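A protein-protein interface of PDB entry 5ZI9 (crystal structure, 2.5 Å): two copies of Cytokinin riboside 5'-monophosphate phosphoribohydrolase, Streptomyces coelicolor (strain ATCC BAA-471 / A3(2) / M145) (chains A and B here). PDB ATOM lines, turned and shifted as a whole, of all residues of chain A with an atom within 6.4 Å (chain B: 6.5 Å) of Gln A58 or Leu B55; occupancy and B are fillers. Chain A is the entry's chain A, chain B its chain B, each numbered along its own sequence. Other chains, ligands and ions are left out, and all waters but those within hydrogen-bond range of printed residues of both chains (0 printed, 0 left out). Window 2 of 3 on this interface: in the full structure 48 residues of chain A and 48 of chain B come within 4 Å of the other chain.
OE1 of Gln A58 sits close to O of Val B54.
Leu B55 touches one residue of chain A. Printed residues of chain A within 4 Å of Ile B57: Phe A61 (3.997 Å). Of the printed residues of chain A, Gln B58 touches Val A54 and Gln A58. The nearest printed residue of chain A that does not touch Leu B55 is Ile A62 (6.6 Å). The nearest printed residue of chain A that does not touch Val B54 is Phe A61 (4.1 Å).
Val A54 touches Gln B58, and with the chains exchanged Gln A58 touches Val B54. Ile A57 touches Phe B61, and with the chains exchanged Phe A61 touches Ile B57. Gln A58 touches Leu B55, but with the chains exchanged Leu A55 does not touch Gln B58 (4.8 Å). Gln A58 touches its own counterpart, Gln B58. Positions printed for both chains: 53, 54, 55, 56, 57, 58, 59, 60 and 61.
Of the 11 printed residues of chain A, 4 touch a printed residue of chain B. Hydrophobic or aromatic side chains of chain A within 4 Å of the printed part of chain B: Val A54, Ile A57 and Phe A61. Along chain A the printed residues that touch a printed residue of chain B span positions 54 to 61. Hydrophobic or aromatic side chains of chain B that line the printed part of chain A: Val B54, Leu B55, Ile B57 and Phe B61. Among the printed residues, no Asp or Glu carboxylate lies within 4 Å of a Lys or Arg side-chain nitrogen of the other chain.
Val A54 touches Gln B58. Ile A57 touches Phe B61. CD2 of Leu B55 touches NE2 of Gln A58 (3.9 Å). CB of Gln B58 touches OE1 of Gln A58, 3.4 Å away. CG2 of Ile B57 touches CZ of Phe A61, at 3.997 Å. Phe A61 touches Phe B61.
The side-chain hydroxyl (OG) of Ser B59 lies within hydrogen-bond range of the backbone carbonyl oxygen (O) of Leu B55, 2.8 Å away.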
ATOM      1  N   ARG A  53      27.192   6.125  11.313  1.00  0.00           N
ATOM      2  CA  ARG A  53      28.203   5.906  12.358  1.00  0.00           C
ATOM      3  C   ARG A  53      28.073   4.498  12.949  1.00  0.00           C
ATOM      4  O   ARG A  53      29.068   3.798  13.114  1.00  0.00           O
ATOM      5  CB  ARG A  53      28.049   6.978  13.469  1.00  0.00           C
ATOM      6  CG  ARG A  53      29.325   7.619  13.982  1.00  0.00           C
ATOM      7  CD  ARG A  53      29.593   9.018  13.426  1.00  0.00           C
ATOM      8  NE  ARG A  53      28.566  10.037  13.744  1.00  0.00           N
ATOM      9  CZ  ARG A  53      28.644  11.358  13.485  1.00  0.00           C
ATOM     10  NH1 ARG A  53      29.712  11.888  12.942  1.00  0.00           N
ATOM     11  NH2 ARG A  53      27.648  12.163  13.766  1.00  0.00           N
ATOM     12  N   VAL A  54      26.843   4.099  13.252  1.00  0.00           N
ATOM     13  CA  VAL A  54      26.550   2.810  13.868  1.00  0.00           C
ATOM     14  C   VAL A  54      26.987   1.687  12.924  1.00  0.00           C
ATOM     15  O   VAL A  54      27.537   0.668  13.359  1.00  0.00           O
ATOM     16  CB  VAL A  54      25.019   2.656  14.172  1.00  0.00           C
ATOM     17  CG1 VAL A  54      24.625   1.217  14.441  1.00  0.00           C
ATOM     18  CG2 VAL A  54      24.589   3.499  15.360  1.00  0.00           C
ATOM     19  N   LEU A  55      26.708   1.869  11.629  1.00  0.00           N
ATOM     20  CA  LEU A  55      27.052   0.888  10.652  1.00  0.00           C
ATOM     21  C   LEU A  55      28.555   0.770  10.503  1.00  0.00           C
ATOM     22  O   LEU A  55      29.036  -0.324  10.266  1.00  0.00           O
ATOM     23  CB  LEU A  55      26.418   1.217   9.304  1.00  0.00           C
ATOM     24  CG  LEU A  55      24.898   1.231   9.256  1.00  0.00           C
ATOM     25  CD1 LEU A  55      24.446   1.641   7.872  1.00  0.00           C
ATOM     26  CD2 LEU A  55      24.263  -0.118   9.632  1.00  0.00           C
ATOM     27  N   ARG A  56      29.299   1.878  10.602  1.00  0.00           N
ATOM     28  CA  ARG A  56      30.765   1.809  10.438  1.00  0.00           C
ATOM     29  C   ARG A  56      31.373   1.223  11.659  1.00  0.00           C
ATOM     30  O   ARG A  56      32.278   0.387  11.561  1.00  0.00           O
ATOM     31  CB  ARG A  56      31.438   3.156  10.109  1.00  0.00           C
ATOM     32  CG  ARG A  56      31.368   3.480   8.628  1.00  0.00           C
ATOM     33  CD  ARG A  56      32.635   4.075   8.057  1.00  0.00           C
ATOM     34  NE  ARG A  56      33.567   3.069   7.499  1.00  0.00           N
ATOM     35  CZ  ARG A  56      34.523   3.305   6.590  1.00  0.00           C
ATOM     36  NH1 ARG A  56      34.706   4.517   6.066  1.00  0.00           N
ATOM     37  NH2 ARG A  56      35.312   2.313   6.183  1.00  0.00           N
ATOM     38  N   ILE A  57      30.856   1.631  12.809  1.00  0.00           N
ATOM     39  CA  ILE A  57      31.383   1.117  14.074  1.00  0.00           C
ATOM     40  C   ILE A  57      31.211  -0.382  14.163  1.00  0.00           C
ATOM     41  O   ILE A  57      32.122  -1.096  14.538  1.00  0.00           O
ATOM     42  CB  ILE A  57      30.731   1.817  15.282  1.00  0.00           C
ATOM     43  CG1 ILE A  57      31.292   3.237  15.404  1.00  0.00           C
ATOM     44  CG2 ILE A  57      31.021   1.077  16.585  1.00  0.00           C
ATOM     45  CD1 ILE A  57      30.416   4.167  16.202  1.00  0.00           C
ATOM     46  N   GLN A  58      30.030  -0.838  13.818  1.00  0.00           N
ATOM     47  CA  GLN A  58      29.682  -2.209  13.959  1.00  0.00           C
ATOM     48  C   GLN A  58      30.511  -3.056  13.004  1.00  0.00           C
ATOM     49  O   GLN A  58      30.923  -4.167  13.351  1.00  0.00           O
ATOM     50  CB  GLN A  58      28.185  -2.383  13.706  1.00  0.00           C
ATOM     51  CG  GLN A  58      27.714  -3.802  13.429  1.00  0.00           C
ATOM     52  CD  GLN A  58      27.627  -4.651  14.674  1.00  0.00           C
ATOM     53  OE1 GLN A  58      28.168  -4.317  15.751  1.00  0.00           O
ATOM     54  NE2 GLN A  58      26.911  -5.773  14.537  1.00  0.00           N
ATOM     55  N   SER A  59      30.787  -2.525  11.823  1.00  0.00           N
ATOM     56  CA  SER A  59      31.570  -3.252  10.874  1.00  0.00           C
ATOM     57  C   SER A  59      33.015  -3.422  11.344  1.00  0.00           C
ATOM     58  O   SER A  59      33.675  -4.386  10.940  1.00  0.00           O
ATOM     59  CB  SER A  59      31.502  -2.598   9.511  1.00  0.00           C
ATOM     60  OG  SER A  59      32.210  -1.394   9.504  1.00  0.00           O
ATOM     61  N   GLU A  60      33.511  -2.515  12.179  1.00  0.00           N
ATOM     62  CA  GLU A  60      34.835  -2.663  12.737  1.00  0.00           C
ATOM     63  C   GLU A  60      34.870  -3.703  13.783  1.00  0.00           C
ATOM     64  O   GLU A  60      35.851  -4.309  13.959  1.00  0.00           O
ATOM     65  CB  GLU A  60      35.338  -1.364  13.369  1.00  0.00           C
ATOM     66  CG  GLU A  60      35.728  -0.328  12.334  1.00  0.00           C
ATOM     67  CD  GLU A  60      36.897   0.532  12.753  1.00  0.00           C
ATOM     68  OE1 GLU A  60      37.261   0.536  13.946  1.00  0.00           O
ATOM     69  OE2 GLU A  60      37.456   1.194  11.859  1.00  0.00           O
ATOM     70  N   PHE A  61      33.811  -3.863  14.531  1.00  0.00           N
ATOM     71  CA  PHE A  61      33.766  -4.935  15.495  1.00  0.00           C
ATOM     72  C   PHE A  61      33.736  -6.299  14.784  1.00  0.00           C
ATOM     73  O   PHE A  61      34.305  -7.261  15.245  1.00  0.00           O
ATOM     74  CB  PHE A  61      32.518  -4.787  16.358  1.00  0.00           C
ATOM     75  CG  PHE A  61      32.678  -3.852  17.509  1.00  0.00           C
ATOM     76  CD1 PHE A  61      33.265  -4.294  18.689  1.00  0.00           C
ATOM     77  CD2 PHE A  61      32.195  -2.568  17.439  1.00  0.00           C
ATOM     78  CE1 PHE A  61      33.385  -3.472  19.783  1.00  0.00           C
ATOM     79  CE2 PHE A  61      32.317  -1.714  18.521  1.00  0.00           C
ATOM     80  CZ  PHE A  61      32.912  -2.170  19.699  1.00  0.00           C
ATOM     81  N   ILE A  62      33.064  -6.360  13.657  1.00  0.00           N
ATOM     82  CA  ILE A  62      32.894  -7.593  12.916  1.00  0.00           C
ATOM     83  C   ILE A  62      34.228  -7.999  12.295  1.00  0.00           C
ATOM     84  O   ILE A  62      34.617  -9.160  12.232  1.00  0.00           O
ATOM     85  CB  ILE A  62      31.756  -7.405  11.860  1.00  0.00           C
ATOM     86  CG1 ILE A  62      30.398  -7.478  12.565  1.00  0.00           C
ATOM     87  CG2 ILE A  62      31.802  -8.410  10.711  1.00  0.00           C
ATOM     88  CD1 ILE A  62      29.359  -6.725  11.766  1.00  0.00           C
ATOM     89  N   GLU A  63      34.938  -6.990  11.874  1.00  0.00           N
ATOM     90  CA  GLU A  63      36.235  -7.163  11.296  1.00  0.00           C
ATOM     91  C   GLU A  63      37.230  -7.652  12.396  1.00  0.00           C
ATOM     92  O   GLU A  63      38.035  -8.581  12.165  1.00  0.00           O
ATOM     93  CB  GLU A  63      36.619  -5.838  10.628  1.00  0.00           C
ATOM     94  CG  GLU A  63      37.346  -6.010   9.349  1.00  0.00           C
ATOM     95  CD  GLU A  63      36.492  -6.386   8.166  1.00  0.00           C
ATOM     96  OE1 GLU A  63      35.692  -5.607   7.661  1.00  0.00           O
ATOM     97  OE2 GLU A  63      36.708  -7.461   7.643  1.00  0.00           O
ATOM     98  N   ASP B  50      29.949 -14.856  20.996  1.00  0.00           N
ATOM     99  CA  ASP B  50      30.373 -13.550  20.478  1.00  0.00           C
ATOM    100  C   ASP B  50      29.570 -12.874  19.322  1.00  0.00           C
ATOM    101  O   ASP B  50      29.437 -11.647  19.334  1.00  0.00           O
ATOM    102  CB  ASP B  50      31.862 -13.570  20.151  1.00  0.00           C
ATOM    103  CG  ASP B  50      32.696 -13.503  21.382  1.00  0.00           C
ATOM    104  OD1 ASP B  50      32.225 -13.029  22.413  1.00  0.00           O
ATOM    105  OD2 ASP B  50      33.830 -13.966  21.337  1.00  0.00           O
ATOM    106  N   PRO B  51      29.079 -13.655  18.331  1.00  0.00           N
ATOM    107  CA  PRO B  51      28.275 -13.059  17.269  1.00  0.00           C
ATOM    108  C   PRO B  51      27.041 -12.400  17.841  1.00  0.00           C
ATOM    109  O   PRO B  51      26.680 -11.368  17.373  1.00  0.00           O
ATOM    110  CB  PRO B  51      27.858 -14.253  16.417  1.00  0.00           C
ATOM    111  CG  PRO B  51      28.892 -15.230  16.665  1.00  0.00           C
ATOM    112  CD  PRO B  51      29.235 -15.098  18.112  1.00  0.00           C
ATOM    113  N   TRP B  52      26.416 -12.993  18.860  1.00  0.00           N
ATOM    114  CA  TRP B  52      25.281 -12.370  19.517  1.00  0.00           C
ATOM    115  C   TRP B  52      25.702 -11.188  20.381  1.00  0.00           C
ATOM    116  O   TRP B  52      24.968 -10.253  20.548  1.00  0.00           O
ATOM    117  CB  TRP B  52      24.529 -13.407  20.382  1.00  0.00           C
ATOM    118  CG  TRP B  52      23.320 -12.816  21.023  1.00  0.00           C
ATOM    119  CD1 TRP B  52      23.192 -12.440  22.327  1.00  0.00           C
ATOM    120  CD2 TRP B  52      22.087 -12.466  20.381  1.00  0.00           C
ATOM    121  NE1 TRP B  52      21.941 -11.908  22.554  1.00  0.00           N
ATOM    122  CE2 TRP B  52      21.249 -11.896  21.371  1.00  0.00           C
ATOM    123  CE3 TRP B  52      21.609 -12.585  19.086  1.00  0.00           C
ATOM    124  CZ2 TRP B  52      19.967 -11.451  21.092  1.00  0.00           C
ATOM    125  CZ3 TRP B  52      20.340 -12.145  18.810  1.00  0.00           C
ATOM    126  CH2 TRP B  52      19.532 -11.569  19.806  1.00  0.00           C
ATOM    127  N   ARG B  53      26.864 -11.270  20.986  1.00  0.00           N
ATOM    128  CA  ARG B  53      27.362 -10.167  21.776  1.00  0.00           C
ATOM    129  C   ARG B  53      27.580  -8.942  20.944  1.00  0.00           C
ATOM    130  O   ARG B  53      27.357  -7.861  21.381  1.00  0.00           O
ATOM    131  CB  ARG B  53      28.667 -10.536  22.461  1.00  0.00           C
ATOM    132  CG  ARG B  53      28.488 -11.487  23.651  1.00  0.00           C
ATOM    133  CD  ARG B  53      29.770 -11.478  24.437  1.00  0.00           C
ATOM    134  NE  ARG B  53      29.659 -12.332  25.598  1.00  0.00           N
ATOM    135  CZ  ARG B  53      29.948 -13.618  25.634  1.00  0.00           C
ATOM    136  NH1 ARG B  53      29.752 -14.291  26.746  1.00  0.00           N
ATOM    137  NH2 ARG B  53      30.439 -14.241  24.574  1.00  0.00           N
ATOM    138  N   VAL B  54      28.000  -9.145  19.723  1.00  0.00           N
ATOM    139  CA  VAL B  54      28.196  -8.072  18.777  1.00  0.00           C
ATOM    140  C   VAL B  54      26.883  -7.326  18.489  1.00  0.00           C
ATOM    141  O   VAL B  54      26.877  -6.125  18.295  1.00  0.00           O
ATOM    142  CB  VAL B  54      28.913  -8.644  17.517  1.00  0.00           C
ATOM    143  CG1 VAL B  54      28.140  -8.407  16.257  1.00  0.00           C
ATOM    144  CG2 VAL B  54      30.263  -8.014  17.364  1.00  0.00           C
ATOM    145  N   LEU B  55      25.776  -8.049  18.442  1.00  0.00           N
ATOM    146  CA  LEU B  55      24.464  -7.439  18.257  1.00  0.00           C
ATOM    147  C   LEU B  55      24.022  -6.666  19.484  1.00  0.00           C
ATOM    148  O   LEU B  55      23.332  -5.677  19.371  1.00  0.00           O
ATOM    149  CB  LEU B  55      23.441  -8.511  17.895  1.00  0.00           C
ATOM    150  CG  LEU B  55      23.666  -9.195  16.531  1.00  0.00           C
ATOM    151  CD1 LEU B  55      22.365  -9.873  16.145  1.00  0.00           C
ATOM    152  CD2 LEU B  55      24.100  -8.265  15.396  1.00  0.00           C
ATOM    153  N   ARG B  56      24.420  -7.153  20.657  1.00  0.00           N
ATOM    154  CA  ARG B  56      24.154  -6.492  21.925  1.00  0.00           C
ATOM    155  C   ARG B  56      24.913  -5.201  22.096  1.00  0.00           C
ATOM    156  O   ARG B  56      24.365  -4.244  22.593  1.00  0.00           O
ATOM    157  CB  ARG B  56      24.551  -7.412  23.085  1.00  0.00           C
ATOM    158  CG  ARG B  56      23.619  -8.586  23.272  1.00  0.00           C
ATOM    159  CD  ARG B  56      22.260  -8.108  23.729  1.00  0.00           C
ATOM    160  NE  ARG B  56      21.794  -8.932  24.828  1.00  0.00           N
ATOM    161  CZ  ARG B  56      20.979  -8.528  25.783  1.00  0.00           C
ATOM    162  NH1 ARG B  56      20.511  -7.295  25.813  1.00  0.00           N
ATOM    163  NH2 ARG B  56      20.618  -9.379  26.731  1.00  0.00           N
ATOM    164  N   ILE B  57      26.185  -5.216  21.721  1.00  0.00           N
ATOM    165  CA  ILE B  57      27.030  -4.057  21.737  1.00  0.00           C
ATOM    166  C   ILE B  57      26.497  -2.985  20.802  1.00  0.00           C
ATOM    167  O   ILE B  57      26.452  -1.826  21.169  1.00  0.00           O
ATOM    168  CB  ILE B  57      28.458  -4.424  21.306  1.00  0.00           C
ATOM    169  CG1 ILE B  57      29.108  -5.270  22.389  1.00  0.00           C
ATOM    170  CG2 ILE B  57      29.307  -3.164  21.110  1.00  0.00           C
ATOM    171  CD1 ILE B  57      30.294  -6.047  21.874  1.00  0.00           C
ATOM    172  N   GLN B  58      26.131  -3.392  19.589  1.00  0.00           N
ATOM    173  CA  GLN B  58      25.559  -2.486  18.618  1.00  0.00           C
ATOM    174  C   GLN B  58      24.271  -1.862  19.145  1.00  0.00           C
ATOM    175  O   GLN B  58      24.045  -0.669  19.001  1.00  0.00           O
ATOM    176  CB  GLN B  58      25.294  -3.221  17.305  1.00  0.00           C
ATOM    177  CG  GLN B  58      24.986  -2.327  16.102  1.00  0.00           C
ATOM    178  CD  GLN B  58      24.214  -3.038  15.006  1.00  0.00           C
ATOM    179  OE1 GLN B  58      23.423  -3.964  15.267  1.00  0.00           O
ATOM    180  NE2 GLN B  58      24.437  -2.625  13.776  1.00  0.00           N
ATOM    181  N   SER B  59      23.424  -2.667  19.773  1.00  0.00           N
ATOM    182  CA  SER B  59      22.206  -2.142  20.399  1.00  0.00           C
ATOM    183  C   SER B  59      22.477  -1.035  21.436  1.00  0.00           C
ATOM    184  O   SER B  59      21.773  -0.022  21.505  1.00  0.00           O
ATOM    185  CB  SER B  59      21.438  -3.264  21.067  1.00  0.00           C
ATOM    186  OG  SER B  59      21.087  -4.192  20.087  1.00  0.00           O
ATOM    187  N   GLU B  60      23.504  -1.252  22.245  1.00  0.00           N
ATOM    188  CA  GLU B  60      23.872  -0.283  23.257  1.00  0.00           C
ATOM    189  C   GLU B  60      24.384   1.015  22.662  1.00  0.00           C
ATOM    190  O   GLU B  60      24.067   2.067  23.169  1.00  0.00           O
ATOM    191  CB  GLU B  60      24.893  -0.849  24.246  1.00  0.00           C
ATOM    192  CG  GLU B  60      25.054   0.111  25.413  1.00  0.00           C
ATOM    193  CD  GLU B  60      25.607  -0.527  26.657  1.00  0.00           C
ATOM    194  OE1 GLU B  60      26.848  -0.529  26.813  1.00  0.00           O
ATOM    195  OE2 GLU B  60      24.808  -0.958  27.506  1.00  0.00           O
ATOM    196  N   PHE B  61      25.146   0.946  21.584  1.00  0.00           N
ATOM    197  CA  PHE B  61      25.501   2.153  20.834  1.00  0.00           C
ATOM    198  C   PHE B  61      24.270   2.858  20.328  1.00  0.00           C
ATOM    199  O   PHE B  61      24.182   4.077  20.431  1.00  0.00           O
ATOM    200  CB  PHE B  61      26.338   1.841  19.608  1.00  0.00           C
ATOM    201  CG  PHE B  61      27.769   1.757  19.883  1.00  0.00           C
ATOM    202  CD1 PHE B  61      28.495   2.901  20.100  1.00  0.00           C
ATOM    203  CD2 PHE B  61      28.403   0.532  19.911  1.00  0.00           C
ATOM    204  CE1 PHE B  61      29.848   2.826  20.362  1.00  0.00           C
ATOM    205  CE2 PHE B  61      29.755   0.442  20.139  1.00  0.00           C
ATOM    206  CZ  PHE B  61      30.490   1.601  20.377  1.00  0.00           C
